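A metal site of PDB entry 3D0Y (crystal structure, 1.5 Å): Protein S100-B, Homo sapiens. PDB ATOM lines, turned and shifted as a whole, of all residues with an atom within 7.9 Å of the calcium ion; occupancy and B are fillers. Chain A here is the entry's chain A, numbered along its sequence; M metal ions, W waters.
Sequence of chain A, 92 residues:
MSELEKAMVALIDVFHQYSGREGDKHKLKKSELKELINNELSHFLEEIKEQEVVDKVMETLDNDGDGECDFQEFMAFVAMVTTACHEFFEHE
The calcium ion is bound by OD1 of Asp 62 (2.2 Å), OD2 of Asp 64 (2.2 Å), O of Glu 68 (2.3 Å), OD1 of Asp 66 (2.3 Å), water W1 (2.3 Å), OE1 of Glu 73 (2.5 Å) and OE2 of Glu 73 (2.6 Å).
Of the 15 residues printed, 5 come within 4 Å of the calcium ion. Along chain A the residues within 4 Å of the calcium ion span positions 62 to 73. The nearest printed residue that does not touch the calcium ion is Cys 69 (4.4 Å).
The backbone NH (N) of Glu 73 sits at hydrogen-bond distance from the side-chain carboxylate (OD1) of Asp 70 (2.8 Å). OD1 of Asp 62 sits close to N of Gly 65 (3.1 Å). The side-chain carboxylate (OE2) of Glu 73 sits close to the backbone NH (N) of Asn 63 (3.0 Å). The side-chain carboxylate of Asp 62 sits at hydrogen-bond distance from the backbone NH of Gly 67, at 2.7 Å.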
ATOM      1  N   LYS A  27     -10.908  23.268   3.937  1.00  0.00           N
ATOM      2  CA  LYS A  27      -9.773  23.887   4.578  1.00  0.00           C
ATOM      3  C   LYS A  27      -8.525  23.811   3.693  1.00  0.00           C
ATOM      4  O   LYS A  27      -8.335  22.846   2.922  1.00  0.00           O
ATOM      5  CB  LYS A  27      -9.495  23.197   5.928  1.00  0.00           C
ATOM      6  CG  LYS A  27     -10.582  23.422   6.971  1.00  0.00           C
ATOM      7  CD  LYS A  27     -10.164  22.889   8.310  1.00  0.00           C
ATOM      8  CE  LYS A  27     -11.385  22.802   9.253  1.00  0.00           C
ATOM      9  NZ  LYS A  27     -12.577  22.155   8.606  1.00  0.00           N
ATOM     10  N   LEU A  28      -7.704  24.854   3.820  1.00  0.00           N
ATOM     11  CA  LEU A  28      -6.358  24.904   3.278  1.00  0.00           C
ATOM     12  C   LEU A  28      -5.366  24.269   4.258  1.00  0.00           C
ATOM     13  O   LEU A  28      -5.242  24.740   5.373  1.00  0.00           O
ATOM     14  CB  LEU A  28      -5.964  26.378   2.989  1.00  0.00           C
ATOM     15  CG  LEU A  28      -6.764  27.170   1.924  1.00  0.00           C
ATOM     16  CD1 LEU A  28      -6.451  28.663   1.943  1.00  0.00           C
ATOM     17  CD2 LEU A  28      -6.607  26.567   0.514  1.00  0.00           C
ATOM     18  N   MET A  58       0.875  30.063   7.968  1.00  0.00           N
ATOM     19  CA  MET A  58      -0.161  29.292   8.613  1.00  0.00           C
ATOM     20  C   MET A  58      -0.296  29.612  10.100  1.00  0.00           C
ATOM     21  O   MET A  58      -1.410  29.683  10.613  1.00  0.00           O
ATOM     22  CB  MET A  58       0.096  27.802   8.447  1.00  0.00           C
ATOM     23  CG  MET A  58      -1.081  26.953   9.012  1.00  0.00           C
ATOM     24  SD  MET A  58      -2.574  27.183   8.032  1.00  0.00           S
ATOM     25  CE  MET A  58      -2.222  26.228   6.555  1.00  0.00           C
ATOM     26  N   LEU A  61      -2.174  32.798  10.404  1.00  0.00           N
ATOM     27  CA  LEU A  61      -3.554  32.716   9.925  1.00  0.00           C
ATOM     28  C   LEU A  61      -4.467  31.839  10.760  1.00  0.00           C
ATOM     29  O   LEU A  61      -5.666  32.087  10.859  1.00  0.00           O
ATOM     30  CB  LEU A  61      -3.562  32.204   8.489  1.00  0.00           C
ATOM     31  CG  LEU A  61      -3.113  33.242   7.452  1.00  0.00           C
ATOM     32  CD1 LEU A  61      -3.232  32.688   6.055  1.00  0.00           C
ATOM     33  CD2 LEU A  61      -3.829  34.610   7.635  1.00  0.00           C
ATOM     34  N   ASP A  62      -3.887  30.807  11.371  1.00  0.00           N
ATOM     35  CA  ASP A  62      -4.644  29.733  12.022  1.00  0.00           C
ATOM     36  C   ASP A  62      -5.088  30.045  13.464  1.00  0.00           C
ATOM     37  O   ASP A  62      -4.467  29.606  14.435  1.00  0.00           O
ATOM     38  CB  ASP A  62      -3.855  28.415  11.953  1.00  0.00           C
ATOM     39  CG  ASP A  62      -4.560  27.278  12.640  1.00  0.00           C
ATOM     40  OD1 ASP A  62      -5.802  27.279  12.631  1.00  0.00           O
ATOM     41  OD2 ASP A  62      -3.860  26.374  13.161  1.00  0.00           O
ATOM     42  N   ASN A  63      -6.225  30.725  13.569  1.00  0.00           N
ATOM     43  CA  ASN A  63      -6.741  31.234  14.827  1.00  0.00           C
ATOM     44  C   ASN A  63      -7.366  30.175  15.718  1.00  0.00           C
ATOM     45  O   ASN A  63      -7.415  30.333  16.947  1.00  0.00           O
ATOM     46  CB  ASN A  63      -7.742  32.341  14.541  1.00  0.00           C
ATOM     47  CG  ASN A  63      -7.104  33.527  13.830  1.00  0.00           C
ATOM     48  OD1 ASN A  63      -6.097  34.060  14.291  1.00  0.00           O
ATOM     49  ND2 ASN A  63      -7.689  33.931  12.696  1.00  0.00           N
ATOM     50  N   ASP A  64      -7.857  29.092  15.113  1.00  0.00           N
ATOM     51  CA  ASP A  64      -8.418  28.005  15.898  1.00  0.00           C
ATOM     52  C   ASP A  64      -7.455  26.849  16.157  1.00  0.00           C
ATOM     53  O   ASP A  64      -7.848  25.834  16.748  1.00  0.00           O
ATOM     54  CB  ASP A  64      -9.753  27.520  15.334  1.00  0.00           C
ATOM     55  CG  ASP A  64      -9.623  26.797  14.027  1.00  0.00           C
ATOM     56  OD1 ASP A  64     -10.644  26.355  13.487  1.00  0.00           O
ATOM     57  OD2 ASP A  64      -8.498  26.648  13.543  1.00  0.00           O
ATOM     58  N   GLY A  65      -6.198  26.998  15.743  1.00  0.00           N
ATOM     59  CA  GLY A  65      -5.137  26.033  16.075  1.00  0.00           C
ATOM     60  C   GLY A  65      -5.213  24.613  15.505  1.00  0.00           C
ATOM     61  O   GLY A  65      -4.552  23.724  16.060  1.00  0.00           O
ATOM     62  N   ASP A  66      -5.980  24.373  14.433  1.00  0.00           N
ATOM     63  CA  ASP A  66      -6.075  23.024  13.805  1.00  0.00           C
ATOM     64  C   ASP A  66      -5.051  22.828  12.687  1.00  0.00           C
ATOM     65  O   ASP A  66      -5.116  21.847  11.926  1.00  0.00           O
ATOM     66  CB  ASP A  66      -7.506  22.722  13.289  1.00  0.00           C
ATOM     67  CG  ASP A  66      -7.912  23.608  12.111  1.00  0.00           C
ATOM     68  OD1 ASP A  66      -7.182  24.581  11.813  1.00  0.00           O
ATOM     69  OD2 ASP A  66      -8.977  23.372  11.485  1.00  0.00           O
ATOM     70  N   GLY A  67      -4.106  23.745  12.592  1.00  0.00           N
ATOM     71  CA  GLY A  67      -3.092  23.732  11.545  1.00  0.00           C
ATOM     72  C   GLY A  67      -3.579  23.904  10.111  1.00  0.00           C
ATOM     73  O   GLY A  67      -2.813  23.706   9.154  1.00  0.00           O
ATOM     74  N   GLU A  68      -4.837  24.302   9.944  1.00  0.00           N
ATOM     75  CA  GLU A  68      -5.359  24.558   8.613  1.00  0.00           C
ATOM     76  C   GLU A  68      -6.027  25.906   8.592  1.00  0.00           C
ATOM     77  O   GLU A  68      -6.368  26.452   9.655  1.00  0.00           O
ATOM     78  CB  GLU A  68      -6.418  23.530   8.175  1.00  0.00           C
ATOM     79  CG  GLU A  68      -6.059  22.116   8.483  1.00  0.00           C
ATOM     80  CD  GLU A  68      -6.039  21.187   7.284  1.00  0.00           C
ATOM     81  OE1 GLU A  68      -6.755  21.434   6.280  1.00  0.00           O
ATOM     82  OE2 GLU A  68      -5.292  20.186   7.340  1.00  0.00           O
ATOM     83  N   CYS A  69      -6.200  26.418   7.373  1.00  0.00           N
ATOM     84  CA  CYS A  69      -6.878  27.689   7.152  1.00  0.00           C
ATOM     85  C   CYS A  69      -8.274  27.436   6.634  1.00  0.00           C
ATOM     86  O   CYS A  69      -8.441  26.937   5.512  1.00  0.00           O
ATOM     87  CB  CYS A  69      -6.105  28.551   6.158  1.00  0.00           C
ATOM     88  SG  CYS A  69      -6.838  30.168   5.882  1.00  0.00           S
ATOM     89  N   ASP A  70      -9.279  27.733   7.459  1.00  0.00           N
ATOM     90  CA  ASP A  70     -10.674  27.544   7.051  1.00  0.00           C
ATOM     91  C   ASP A  70     -11.200  28.795   6.336  1.00  0.00           C
ATOM     92  O   ASP A  70     -10.445  29.719   6.076  1.00  0.00           O
ATOM     93  CB  ASP A  70     -11.584  27.097   8.208  1.00  0.00           C
ATOM     94  CG  ASP A  70     -11.771  28.167   9.280  1.00  0.00           C
ATOM     95  OD1 ASP A  70     -11.427  29.336   9.135  1.00  0.00           O
ATOM     96  OD2 ASP A  70     -12.320  27.836  10.358  1.00  0.00           O
ATOM     97  N   PHE A  71     -12.459  28.812   5.947  1.00  0.00           N
ATOM     98  CA  PHE A  71     -12.954  29.930   5.169  1.00  0.00           C
ATOM     99  C   PHE A  71     -12.913  31.242   5.932  1.00  0.00           C
ATOM    100  O   PHE A  71     -12.466  32.236   5.386  1.00  0.00           O
ATOM    101  CB  PHE A  71     -14.366  29.691   4.632  1.00  0.00           C
ATOM    102  CG  PHE A  71     -14.785  30.746   3.656  1.00  0.00           C
ATOM    103  CD1 PHE A  71     -14.268  30.739   2.349  1.00  0.00           C
ATOM    104  CD2 PHE A  71     -15.645  31.795   4.050  1.00  0.00           C
ATOM    105  CE1 PHE A  71     -14.625  31.738   1.428  1.00  0.00           C
ATOM    106  CE2 PHE A  71     -16.007  32.772   3.150  1.00  0.00           C
ATOM    107  CZ  PHE A  71     -15.483  32.772   1.843  1.00  0.00           C
ATOM    108  N   GLU A  73     -10.897  32.035   8.408  1.00  0.00           N
ATOM    109  CA  GLU A  73      -9.486  32.431   8.424  1.00  0.00           C
ATOM    110  C   GLU A  73      -8.967  32.940   7.078  1.00  0.00           C
ATOM    111  O   GLU A  73      -8.101  33.814   7.060  1.00  0.00           O
ATOM    112  CB  GLU A  73      -8.645  31.245   8.913  1.00  0.00           C
ATOM    113  CG  GLU A  73      -8.822  30.971  10.382  1.00  0.00           C
ATOM    114  CD  GLU A  73      -8.485  29.571  10.761  1.00  0.00           C
ATOM    115  OE1 GLU A  73      -8.374  28.648   9.896  1.00  0.00           O
ATOM    116  OE2 GLU A  73      -8.349  29.334  11.983  1.00  0.00           O
HETATM  117 CA    CA M   1      -7.630  26.857  11.506  1.00  0.00          CA
HETATM  118  O   HOH W   1      -9.655  25.902  10.806  1.00  0.00           O
